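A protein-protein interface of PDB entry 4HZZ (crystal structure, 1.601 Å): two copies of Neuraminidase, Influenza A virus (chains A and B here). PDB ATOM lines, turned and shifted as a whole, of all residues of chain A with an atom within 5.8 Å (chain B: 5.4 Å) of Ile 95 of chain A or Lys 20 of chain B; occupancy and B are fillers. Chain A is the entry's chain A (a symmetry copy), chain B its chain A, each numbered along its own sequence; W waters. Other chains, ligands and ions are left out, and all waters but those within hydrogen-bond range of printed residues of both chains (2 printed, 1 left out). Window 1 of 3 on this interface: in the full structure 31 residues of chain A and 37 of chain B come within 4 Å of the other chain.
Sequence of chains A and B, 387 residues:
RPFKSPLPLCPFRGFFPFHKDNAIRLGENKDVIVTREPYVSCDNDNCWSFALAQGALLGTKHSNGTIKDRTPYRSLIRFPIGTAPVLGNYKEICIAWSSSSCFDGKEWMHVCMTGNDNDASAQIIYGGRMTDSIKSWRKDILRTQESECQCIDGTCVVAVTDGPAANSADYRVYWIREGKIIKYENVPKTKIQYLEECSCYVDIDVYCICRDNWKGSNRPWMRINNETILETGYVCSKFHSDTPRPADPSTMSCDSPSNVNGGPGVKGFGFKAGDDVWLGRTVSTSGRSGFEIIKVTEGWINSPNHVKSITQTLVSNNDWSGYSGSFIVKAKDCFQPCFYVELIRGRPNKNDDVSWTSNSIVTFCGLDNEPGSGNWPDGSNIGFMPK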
ATOM      1  N   PRO A  72     -14.951  -1.565 -14.284  1.00  0.00           N
ATOM      2  CA  PRO A  72     -14.725  -0.165 -14.669  1.00  0.00           C
ATOM      3  C   PRO A  72     -14.494   0.000 -16.166  1.00  0.00           C
ATOM      4  O   PRO A  72     -14.466   1.143 -16.659  1.00  0.00           O
ATOM      5  CB  PRO A  72     -13.432   0.199 -13.935  1.00  0.00           C
ATOM      6  CG  PRO A  72     -13.252  -0.865 -12.871  1.00  0.00           C
ATOM      7  CD  PRO A  72     -13.873  -2.099 -13.433  1.00  0.00           C
ATOM      8  N   TYR A  73     -14.336  -1.118 -16.875  1.00  0.00           N
ATOM      9  CA  TYR A  73     -13.932  -1.101 -18.289  1.00  0.00           C
ATOM     10  C   TYR A  73     -15.125  -1.217 -19.206  1.00  0.00           C
ATOM     11  O   TYR A  73     -14.961  -1.359 -20.413  1.00  0.00           O
ATOM     12  CB  TYR A  73     -12.926  -2.229 -18.578  1.00  0.00           C
ATOM     13  CG  TYR A  73     -11.964  -2.386 -17.428  1.00  0.00           C
ATOM     14  CD1 TYR A  73     -11.177  -1.314 -17.021  1.00  0.00           C
ATOM     15  CD2 TYR A  73     -11.883  -3.570 -16.712  1.00  0.00           C
ATOM     16  CE1 TYR A  73     -10.343  -1.418 -15.956  1.00  0.00           C
ATOM     17  CE2 TYR A  73     -11.032  -3.685 -15.631  1.00  0.00           C
ATOM     18  CZ  TYR A  73     -10.272  -2.605 -15.259  1.00  0.00           C
ATOM     19  OH  TYR A  73      -9.417  -2.697 -14.177  1.00  0.00           O
ATOM     20  N   ARG A  74     -16.321  -1.173 -18.623  1.00  0.00           N
ATOM     21  CA  ARG A  74     -17.552  -1.175 -19.408  1.00  0.00           C
ATOM     22  C   ARG A  74     -17.989   0.256 -19.702  1.00  0.00           C
ATOM     23  O   ARG A  74     -17.952   1.129 -18.829  1.00  0.00           O
ATOM     24  CB  ARG A  74     -18.667  -1.950 -18.691  1.00  0.00           C
ATOM     25  CG  ARG A  74     -18.289  -3.404 -18.387  1.00  0.00           C
ATOM     26  CD  ARG A  74     -19.539  -4.246 -18.181  1.00  0.00           C
ATOM     27  NE  ARG A  74     -20.201  -4.548 -19.454  1.00  0.00           N
ATOM     28  CZ  ARG A  74     -21.205  -5.412 -19.566  1.00  0.00           C
ATOM     29  NH1 ARG A  74     -21.651  -6.034 -18.481  1.00  0.00           N
ATOM     30  NH2 ARG A  74     -21.748  -5.665 -20.756  1.00  0.00           N
ATOM     31  N   SER A  75     -18.381   0.484 -20.956  1.00  0.00           N
ATOM     32  CA  SER A  75     -18.940   1.757 -21.384  1.00  0.00           C
ATOM     33  C   SER A  75     -20.193   1.502 -22.190  1.00  0.00           C
ATOM     34  O   SER A  75     -20.302   0.494 -22.891  1.00  0.00           O
ATOM     35  CB  SER A  75     -17.965   2.488 -22.307  1.00  0.00           C
ATOM     36  OG  SER A  75     -16.824   2.989 -21.626  1.00  0.00           O
ATOM     37  N   LEU A  76     -21.143   2.425 -22.111  1.00  0.00           N
ATOM     38  CA  LEU A  76     -22.228   2.442 -23.075  1.00  0.00           C
ATOM     39  C   LEU A  76     -21.640   2.905 -24.404  1.00  0.00           C
ATOM     40  O   LEU A  76     -21.004   3.965 -24.478  1.00  0.00           O
ATOM     41  CB  LEU A  76     -23.315   3.417 -22.620  1.00  0.00           C
ATOM     42  CG  LEU A  76     -24.440   3.655 -23.623  1.00  0.00           C
ATOM     43  CD1 LEU A  76     -25.202   2.374 -23.923  1.00  0.00           C
ATOM     44  CD2 LEU A  76     -25.379   4.708 -23.066  1.00  0.00           C
ATOM     45  N   GLU A  92     -18.309   6.135 -27.999  1.00  0.00           N
ATOM     46  CA  GLU A  92     -18.427   5.849 -26.583  1.00  0.00           C
ATOM     47  C   GLU A  92     -19.293   6.936 -25.957  1.00  0.00           C
ATOM     48  O   GLU A  92     -18.983   8.126 -26.056  1.00  0.00           O
ATOM     49  CB  GLU A  92     -17.043   5.778 -25.917  1.00  0.00           C
ATOM     50  CG  GLU A  92     -17.056   5.101 -24.530  1.00  0.00           C
ATOM     51  CD  GLU A  92     -16.769   6.039 -23.367  1.00  0.00           C
ATOM     52  OE1 GLU A  92     -16.573   7.248 -23.594  1.00  0.00           O
ATOM     53  OE2 GLU A  92     -16.760   5.564 -22.205  1.00  0.00           O
ATOM     54  N   ILE A  93     -20.404   6.534 -25.355  1.00  0.00           N
ATOM     55  CA  ILE A  93     -21.352   7.498 -24.800  1.00  0.00           C
ATOM     56  C   ILE A  93     -20.992   7.912 -23.370  1.00  0.00           C
ATOM     57  O   ILE A  93     -21.019   9.099 -23.017  1.00  0.00           O
ATOM     58  CB  ILE A  93     -22.795   6.945 -24.816  1.00  0.00           C
ATOM     59  CG1 ILE A  93     -23.185   6.515 -26.237  1.00  0.00           C
ATOM     60  CG2 ILE A  93     -23.776   7.995 -24.272  1.00  0.00           C
ATOM     61  CD1 ILE A  93     -23.161   7.648 -27.260  1.00  0.00           C
ATOM     62  N   CYS A  94     -20.659   6.928 -22.540  1.00  0.00           N
ATOM     63  CA  CYS A  94     -20.290   7.188 -21.157  1.00  0.00           C
ATOM     64  C   CYS A  94     -19.791   5.911 -20.533  1.00  0.00           C
ATOM     65  O   CYS A  94     -20.050   4.828 -21.054  1.00  0.00           O
ATOM     66  CB  CYS A  94     -21.515   7.647 -20.370  1.00  0.00           C
ATOM     67  SG  CYS A  94     -22.859   6.408 -20.491  1.00  0.00           S
ATOM     68  N   ILE A  95     -19.081   6.047 -19.416  1.00  0.00           N
ATOM     69  CA  ILE A  95     -18.678   4.891 -18.614  1.00  0.00           C
ATOM     70  C   ILE A  95     -19.929   4.338 -17.956  1.00  0.00           C
ATOM     71  O   ILE A  95     -20.670   5.076 -17.327  1.00  0.00           O
ATOM     72  CB  ILE A  95     -17.663   5.312 -17.540  1.00  0.00           C
ATOM     73  CG1 ILE A  95     -16.455   6.003 -18.194  1.00  0.00           C
ATOM     74  CG2 ILE A  95     -17.224   4.096 -16.711  1.00  0.00           C
ATOM     75  CD1 ILE A  95     -15.553   6.722 -17.186  1.00  0.00           C
ATOM     76  N   ALA A  96     -20.182   3.042 -18.116  1.00  0.00           N
ATOM     77  CA  ALA A  96     -21.426   2.454 -17.608  1.00  0.00           C
ATOM     78  C   ALA A  96     -21.384   0.934 -17.568  1.00  0.00           C
ATOM     79  O   ALA A  96     -20.969   0.284 -18.524  1.00  0.00           O
ATOM     80  CB  ALA A  96     -22.627   2.909 -18.458  1.00  0.00           C
ATOM     81  N   TRP A  97     -21.861   0.373 -16.460  1.00  0.00           N
ATOM     82  CA  TRP A  97     -22.229  -1.041 -16.432  1.00  0.00           C
ATOM     83  C   TRP A  97     -23.735  -1.279 -16.284  1.00  0.00           C
ATOM     84  O   TRP A  97     -24.176  -2.414 -16.114  1.00  0.00           O
ATOM     85  CB  TRP A  97     -21.407  -1.861 -15.410  1.00  0.00           C
ATOM     86  CG  TRP A  97     -21.205  -1.271 -14.020  1.00  0.00           C
ATOM     87  CD1 TRP A  97     -20.016  -0.922 -13.455  1.00  0.00           C
ATOM     88  CD2 TRP A  97     -22.215  -1.006 -13.024  1.00  0.00           C
ATOM     89  NE1 TRP A  97     -20.211  -0.448 -12.176  1.00  0.00           N
ATOM     90  CE2 TRP A  97     -21.551  -0.481 -11.889  1.00  0.00           C
ATOM     91  CE3 TRP A  97     -23.606  -1.139 -12.989  1.00  0.00           C
ATOM     92  CZ2 TRP A  97     -22.232  -0.104 -10.726  1.00  0.00           C
ATOM     93  CZ3 TRP A  97     -24.289  -0.767 -11.829  1.00  0.00           C
ATOM     94  CH2 TRP A  97     -23.593  -0.244 -10.711  1.00  0.00           C
ATOM     95  N   CYS A 112     -26.183   6.666 -16.988  1.00  0.00           N
ATOM     96  CA  CYS A 112     -25.024   5.767 -16.974  1.00  0.00           C
ATOM     97  C   CYS A 112     -24.577   5.462 -15.561  1.00  0.00           C
ATOM     98  O   CYS A 112     -24.105   6.354 -14.870  1.00  0.00           O
ATOM     99  CB  CYS A 112     -23.860   6.454 -17.682  1.00  0.00           C
ATOM    100  SG  CYS A 112     -24.332   7.118 -19.314  1.00  0.00           S
ATOM    101  N   MET A 113     -24.681   4.209 -15.128  1.00  0.00           N
ATOM    102  CA  MET A 113     -24.228   3.852 -13.782  1.00  0.00           C
ATOM    103  C   MET A 113     -22.857   3.205 -13.818  1.00  0.00           C
ATOM    104  O   MET A 113     -22.601   2.303 -14.635  1.00  0.00           O
ATOM    105  CB  MET A 113     -25.195   2.889 -13.084  1.00  0.00           C
ATOM    106  CG  MET A 113     -26.437   3.522 -12.488  1.00  0.00           C
ATOM    107  SD  MET A 113     -27.610   4.072 -13.745  1.00  0.00           S
ATOM    108  CE  MET A 113     -29.049   4.356 -12.699  1.00  0.00           C
ATOM    109  N   THR A 114     -21.982   3.636 -12.911  1.00  0.00           N
ATOM    110  CA  THR A 114     -20.689   2.989 -12.790  1.00  0.00           C
ATOM    111  C   THR A 114     -20.114   3.228 -11.399  1.00  0.00           C
ATOM    112  O   THR A 114     -20.673   4.015 -10.625  1.00  0.00           O
ATOM    113  CB  THR A 114     -19.730   3.467 -13.900  1.00  0.00           C
ATOM    114  OG1 THR A 114     -18.494   2.755 -13.800  1.00  0.00           O
ATOM    115  CG2 THR A 114     -19.480   4.961 -13.756  1.00  0.00           C
ATOM    116  N   GLN A 123     -24.655   8.947 -13.941  1.00  0.00           N
ATOM    117  CA  GLN A 123     -24.378  10.206 -14.611  1.00  0.00           C
ATOM    118  C   GLN A 123     -25.454  10.426 -15.646  1.00  0.00           C
ATOM    119  O   GLN A 123     -25.801   9.505 -16.390  1.00  0.00           O
ATOM    120  CB  GLN A 123     -23.006  10.172 -15.287  1.00  0.00           C
ATOM    121  CG  GLN A 123     -21.842  10.286 -14.305  1.00  0.00           C
ATOM    122  CD  GLN A 123     -21.887   9.206 -13.242  1.00  0.00           C
ATOM    123  OE1 GLN A 123     -22.100   9.489 -12.060  1.00  0.00           O
ATOM    124  NE2 GLN A 123     -21.700   7.954 -13.662  1.00  0.00           N
ATOM    125  N   PRO B  17     -17.479  10.228 -13.151  1.00  0.00           N
ATOM    126  CA  PRO B  17     -16.861   9.563 -14.306  1.00  0.00           C
ATOM    127  C   PRO B  17     -17.648   9.798 -15.593  1.00  0.00           C
ATOM    128  O   PRO B  17     -18.861   9.602 -15.619  1.00  0.00           O
ATOM    129  CB  PRO B  17     -16.888   8.082 -13.915  1.00  0.00           C
ATOM    130  CG  PRO B  17     -18.035   7.975 -12.945  1.00  0.00           C
ATOM    131  CD  PRO B  17     -18.027   9.269 -12.173  1.00  0.00           C
ATOM    132  N   PHE B  18     -16.934  10.193 -16.648  1.00  0.00           N
ATOM    133  CA  PHE B  18     -17.536  10.673 -17.896  1.00  0.00           C
ATOM    134  C   PHE B  18     -17.268   9.668 -19.028  1.00  0.00           C
ATOM    135  O   PHE B  18     -18.097   8.797 -19.290  1.00  0.00           O
ATOM    136  CB  PHE B  18     -16.909  12.046 -18.190  1.00  0.00           C
ATOM    137  CG  PHE B  18     -17.579  12.863 -19.278  1.00  0.00           C
ATOM    138  CD1 PHE B  18     -18.908  12.700 -19.622  1.00  0.00           C
ATOM    139  CD2 PHE B  18     -16.850  13.866 -19.922  1.00  0.00           C
ATOM    140  CE1 PHE B  18     -19.504  13.511 -20.620  1.00  0.00           C
ATOM    141  CE2 PHE B  18     -17.434  14.671 -20.895  1.00  0.00           C
ATOM    142  CZ  PHE B  18     -18.760  14.483 -21.248  1.00  0.00           C
ATOM    143  N   HIS B  19     -16.105   9.780 -19.673  1.00  0.00           N
ATOM    144  CA  HIS B  19     -15.716   8.903 -20.784  1.00  0.00           C
ATOM    145  C   HIS B  19     -14.434   8.145 -20.435  1.00  0.00           C
ATOM    146  O   HIS B  19     -13.558   8.689 -19.751  1.00  0.00           O
ATOM    147  CB  HIS B  19     -15.428   9.734 -22.046  1.00  0.00           C
ATOM    148  CG  HIS B  19     -16.641  10.349 -22.680  1.00  0.00           C
ATOM    149  ND1 HIS B  19     -17.453   9.670 -23.566  1.00  0.00           N
ATOM    150  CD2 HIS B  19     -17.144  11.604 -22.599  1.00  0.00           C
ATOM    151  CE1 HIS B  19     -18.425  10.470 -23.968  1.00  0.00           C
ATOM    152  NE2 HIS B  19     -18.264  11.650 -23.392  1.00  0.00           N
ATOM    153  N   LYS B  20     -14.306   6.903 -20.907  1.00  0.00           N
ATOM    154  CA  LYS B  20     -13.091   6.116 -20.701  1.00  0.00           C
ATOM    155  C   LYS B  20     -12.820   5.282 -21.939  1.00  0.00           C
ATOM    156  O   LYS B  20     -13.715   4.586 -22.425  1.00  0.00           O
ATOM    157  CB  LYS B  20     -13.246   5.204 -19.481  1.00  0.00           C
ATOM    158  CG  LYS B  20     -11.986   4.420 -19.122  1.00  0.00           C
ATOM    159  CD  LYS B  20     -12.279   3.448 -17.979  1.00  0.00           C
ATOM    160  CE  LYS B  20     -10.993   2.908 -17.349  1.00  0.00           C
ATOM    161  NZ  LYS B  20     -10.125   2.211 -18.361  1.00  0.00           N
ATOM    162  N   ASP B  21     -11.598   5.331 -22.475  1.00  0.00           N
ATOM    163  CA  ASP B  21     -11.414   4.664 -23.767  1.00  0.00           C
ATOM    164  C   ASP B  21     -10.889   3.229 -23.741  1.00  0.00           C
ATOM    165  O   ASP B  21     -11.062   2.506 -24.725  1.00  0.00           O
ATOM    166  CB  ASP B  21     -10.651   5.525 -24.775  1.00  0.00           C
ATOM    167  CG  ASP B  21      -9.237   5.818 -24.355  1.00  0.00           C
ATOM    168  OD1 ASP B  21      -8.667   5.090 -23.516  1.00  0.00           O
ATOM    169  OD2 ASP B  21      -8.669   6.786 -24.916  1.00  0.00           O
ATOM    170  N   ASN B  22     -10.272   2.807 -22.639  1.00  0.00           N
ATOM    171  CA  ASN B  22      -9.804   1.425 -22.550  1.00  0.00           C
ATOM    172  C   ASN B  22      -8.899   1.091 -23.742  1.00  0.00           C
ATOM    173  O   ASN B  22      -8.869  -0.049 -24.245  1.00  0.00           O
ATOM    174  CB  ASN B  22     -11.000   0.460 -22.506  1.00  0.00           C
ATOM    175  CG  ASN B  22     -11.893   0.698 -21.309  1.00  0.00           C
ATOM    176  OD1 ASN B  22     -13.046   1.135 -21.442  1.00  0.00           O
ATOM    177  ND2 ASN B  22     -11.365   0.439 -20.136  1.00  0.00           N
ATOM    178  N   GLY B  82     -13.453   9.133 -25.760  1.00  0.00           N
ATOM    179  CA  GLY B  82     -13.739   7.844 -25.161  1.00  0.00           C
ATOM    180  C   GLY B  82     -13.596   6.661 -26.106  1.00  0.00           C
ATOM    181  O   GLY B  82     -13.812   5.522 -25.695  1.00  0.00           O
ATOM    182  N   LEU B 343      -3.365   7.436 -18.573  1.00  0.00           N
ATOM    183  CA  LEU B 343      -3.010   6.198 -17.892  1.00  0.00           C
ATOM    184  C   LEU B 343      -1.903   5.532 -18.705  1.00  0.00           C
ATOM    185  O   LEU B 343      -2.171   4.854 -19.695  1.00  0.00           O
ATOM    186  CB  LEU B 343      -4.251   5.304 -17.761  1.00  0.00           C
ATOM    187  CG  LEU B 343      -5.460   6.024 -17.155  1.00  0.00           C
ATOM    188  CD1 LEU B 343      -6.730   5.180 -17.289  1.00  0.00           C
ATOM    189  CD2 LEU B 343      -5.199   6.404 -15.694  1.00  0.00           C
ATOM    190  N   SER B 360      -3.893   5.008 -22.078  1.00  0.00           N
ATOM    191  CA  SER B 360      -5.323   5.174 -22.302  1.00  0.00           C
ATOM    192  C   SER B 360      -5.769   6.437 -21.583  1.00  0.00           C
ATOM    193  O   SER B 360      -4.953   7.142 -20.984  1.00  0.00           O
ATOM    194  CB  SER B 360      -6.117   3.933 -21.860  1.00  0.00           C
ATOM    195  OG  SER B 360      -6.107   3.782 -20.450  1.00  0.00           O
ATOM    196  N   ILE B 361      -7.057   6.737 -21.660  1.00  0.00           N
ATOM    197  CA  ILE B 361      -7.601   7.961 -21.096  1.00  0.00           C
ATOM    198  C   ILE B 361      -8.830   7.655 -20.248  1.00  0.00           C
ATOM    199  O   ILE B 361      -9.627   6.783 -20.588  1.00  0.00           O
ATOM    200  CB  ILE B 361      -8.049   8.937 -22.209  1.00  0.00           C
ATOM    201  CG1 ILE B 361      -6.888   9.268 -23.164  1.00  0.00           C
ATOM    202  CG2 ILE B 361      -8.632  10.214 -21.596  1.00  0.00           C
ATOM    203  CD1 ILE B 361      -7.316  10.056 -24.407  1.00  0.00           C
ATOM    204  N   VAL B 362      -8.982   8.385 -19.149  1.00  0.00           N
ATOM    205  CA  VAL B 362     -10.243   8.414 -18.423  1.00  0.00           C
ATOM    206  C   VAL B 362     -10.566   9.876 -18.100  1.00  0.00           C
ATOM    207  O   VAL B 362      -9.651  10.692 -17.939  1.00  0.00           O
ATOM    208  CB  VAL B 362     -10.193   7.531 -17.154  1.00  0.00           C
ATOM    209  CG1 VAL B 362      -9.144   8.061 -16.155  1.00  0.00           C
ATOM    210  CG2 VAL B 362     -11.580   7.431 -16.533  1.00  0.00           C
ATOM    211  N   THR B 363     -11.844  10.221 -18.044  1.00  0.00           N
ATOM    212  CA  THR B 363     -12.221  11.618 -17.826  1.00  0.00           C
ATOM    213  C   THR B 363     -13.302  11.739 -16.768  1.00  0.00           C
ATOM    214  O   THR B 363     -14.088  10.805 -16.555  1.00  0.00           O
ATOM    215  CB  THR B 363     -12.748  12.283 -19.106  1.00  0.00           C
ATOM    216  OG1 THR B 363     -13.877  11.546 -19.598  1.00  0.00           O
ATOM    217  CG2 THR B 363     -11.685  12.317 -20.188  1.00  0.00           C
ATOM    218  N   TRP B 376     -11.184   3.576 -11.753  1.00  0.00           N
ATOM    219  CA  TRP B 376     -11.215   3.470 -13.212  1.00  0.00           C
ATOM    220  C   TRP B 376      -9.809   3.524 -13.811  1.00  0.00           C
ATOM    221  O   TRP B 376      -9.438   4.496 -14.479  1.00  0.00           O
ATOM    222  CB  TRP B 376     -12.099   4.582 -13.795  1.00  0.00           C
ATOM    223  CG  TRP B 376     -13.534   4.494 -13.360  1.00  0.00           C
ATOM    224  CD1 TRP B 376     -14.545   3.791 -13.975  1.00  0.00           C
ATOM    225  CD2 TRP B 376     -14.123   5.129 -12.221  1.00  0.00           C
ATOM    226  NE1 TRP B 376     -15.720   3.959 -13.281  1.00  0.00           N
ATOM    227  CE2 TRP B 376     -15.491   4.775 -12.203  1.00  0.00           C
ATOM    228  CE3 TRP B 376     -13.631   5.981 -11.221  1.00  0.00           C
ATOM    229  CZ2 TRP B 376     -16.372   5.232 -11.218  1.00  0.00           C
ATOM    230  CZ3 TRP B 376     -14.509   6.431 -10.242  1.00  0.00           C
ATOM    231  CH2 TRP B 376     -15.863   6.060 -10.249  1.00  0.00           C
ATOM    232  N   PRO B 377      -9.012   2.474 -13.565  1.00  0.00           N
ATOM    233  CA  PRO B 377      -7.634   2.402 -14.053  1.00  0.00           C
ATOM    234  C   PRO B 377      -7.580   1.931 -15.502  1.00  0.00           C
ATOM    235  O   PRO B 377      -8.624   1.632 -16.097  1.00  0.00           O
ATOM    236  CB  PRO B 377      -7.018   1.346 -13.133  1.00  0.00           C
ATOM    237  CG  PRO B 377      -8.156   0.389 -12.938  1.00  0.00           C
ATOM    238  CD  PRO B 377      -9.356   1.300 -12.741  1.00  0.00           C
ATOM    239  N   ASP B 378      -6.380   1.858 -16.067  1.00  0.00           N
ATOM    240  CA  ASP B 378      -6.232   1.425 -17.447  1.00  0.00           C
ATOM    241  C   ASP B 378      -6.877   0.059 -17.673  1.00  0.00           C
ATOM    242  O   ASP B 378      -7.638  -0.138 -18.627  1.00  0.00           O
ATOM    243  CB  ASP B 378      -4.759   1.387 -17.817  1.00  0.00           C
ATOM    244  CG  ASP B 378      -4.531   0.754 -19.155  1.00  0.00           C
ATOM    245  OD1 ASP B 378      -4.849   1.413 -20.166  1.00  0.00           O
ATOM    246  OD2 ASP B 378      -4.052  -0.398 -19.183  1.00  0.00           O
ATOM    247  N   GLY B 379      -6.565  -0.888 -16.794  1.00  0.00           N
ATOM    248  CA  GLY B 379      -7.227  -2.179 -16.814  1.00  0.00           C
ATOM    249  C   GLY B 379      -6.620  -3.252 -17.699  1.00  0.00           C
ATOM    250  O   GLY B 379      -7.167  -4.357 -17.780  1.00  0.00           O
HETATM  251  O   HOH W   1     -14.892   1.830 -23.647  1.00  0.00           O
HETATM  252  O   HOH W   2     -20.888   7.685 -16.484  1.00  0.00           O
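Water W2 lies within hydrogen-bond range of O of Ile 95 of chain A (2.8 Å), O of Pro 17 of chain B (2.9 Å) and NE2 of Gln 123 of chain A (2.9 Å).
Water W1 lies within hydrogen-bond range of OD1 of Asn 22 of chain B (3.0 Å), OG of Ser 75 of chain A (3.0 Å) and O of Lys 20 of chain B (3.2 Å).
The backbone carbonyl oxygen of Leu 76 of chain A is in hydrogen-bond range of the backbone NH of Ile 93 of chain A, 2.8 Å away.
The side-chain hydroxyl of Ser 75 of chain A is in hydrogen-bond range of the side-chain carboxylate of Glu 92 of chain A.
N of Gln 123 of chain A is in hydrogen-bond range of O of Cys 112 of chain A (2.8 Å).
NZ of Lys 20 of chain B lies close to ND2 of Asn 22 of chain B (2.8 Å).
The backbone carbonyl oxygen (O) of Thr 363 of chain B lies within hydrogen-bond range of the backbone NH (N) of Phe 18 of chain B.
O of Cys 94 of chain A is in hydrogen-bond range of N of Leu 76 of chain A (2.8 Å).
The backbone NH (N) of Ile 95 of chain A sits at hydrogen-bond distance from the backbone carbonyl oxygen (O) of Phe 18 of chain B, at 2.9 Å.
The side-chain carboxylate of Glu 92 of chain A lies within hydrogen-bond range of a ring nitrogen (ND1) of His 19 of chain B, at 2.6 Å.
OD1 of Asn 22 of chain B sits close to O of Tyr 73 of chain A (3.3 Å).
NE1 of Trp 376 of chain B is in hydrogen-bond range of OG1 of Thr 114 of chain A.
N of Lys 20 of chain B is in hydrogen-bond range of OE2 of Glu 92 of chain A.
CB of Pro 72 of chain A touches CD1 of Trp 376 of chain B (3.8 Å).
NZ of Lys 20 of chain B touches CD1 of Tyr 73 of chain A, at 3.9 Å.
Tyr 73 of chain A touches Pro 377 of chain B.
Lys 20 of chain B touches Ser 75 of chain A (O to OG, 3.6 Å).
CB of Glu 92 of chain A touches O of Gly 82 of chain B, at 3.2 Å.
CG1 of Ile 95 of chain A touches C of His 19 of chain B, at 3.7 Å.
Lys 20 of chain B touches Ile 95 of chain A.
Ile 95 of chain A touches Trp 376 of chain B (CG2 to NE1, 3.7 Å).
CG of Pro 17 of chain B touches CG2 of Thr 114 of chain A (3.4 Å).
Pro 17 of chain B touches Gln 123 of chain A (O to CG, 3.3 Å).
Hydrophobic or aromatic side chains of chain B within 4 Å of the printed part of chain A: Pro 17, His 19, Trp 376 and Pro 377.
Hydrophobic or aromatic side chains of chain A within 4 Å of the printed part of chain B: Pro 72, Tyr 73 and Ile 95.
Along chain A the printed residues that touch a printed residue of chain B span positions 72 to 123.
No position is printed for both chains.
Ile 95 of chain A touches just these residues of chain B: Pro 17, Phe 18, His 19, Lys 20 and Trp 376.
Of chain A, only Pro 72, Tyr 73, Ser 75, Glu 92 and Ile 95 come within 4 Å of Lys 20 of chain B.
Of the printed residues of chain A, His 19 of chain B touches Glu 92, Ile 93 and Ile 95.
Of the printed residues of chain A, Pro 377 of chain B touches Tyr 73 (3.5 Å).
Printed residues of chain A within 4 Å of Trp 376 of chain B: Pro 72 (3.8 Å), Ile 95 (3.7 Å) and Thr 114 (3.1 Å).
Asp 21 of chain B touches none of the printed residues of chain A.
Arg 74 of chain A touches none of the printed residues of chain B.
The nearest residue of chain B that does not touch Ile 95 of chain A is Val 362 of chain B (4.1 Å).
The nearest printed residue of chain A that does not touch Gly 379 of chain B is Pro 72 of chain A (7.2 Å).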
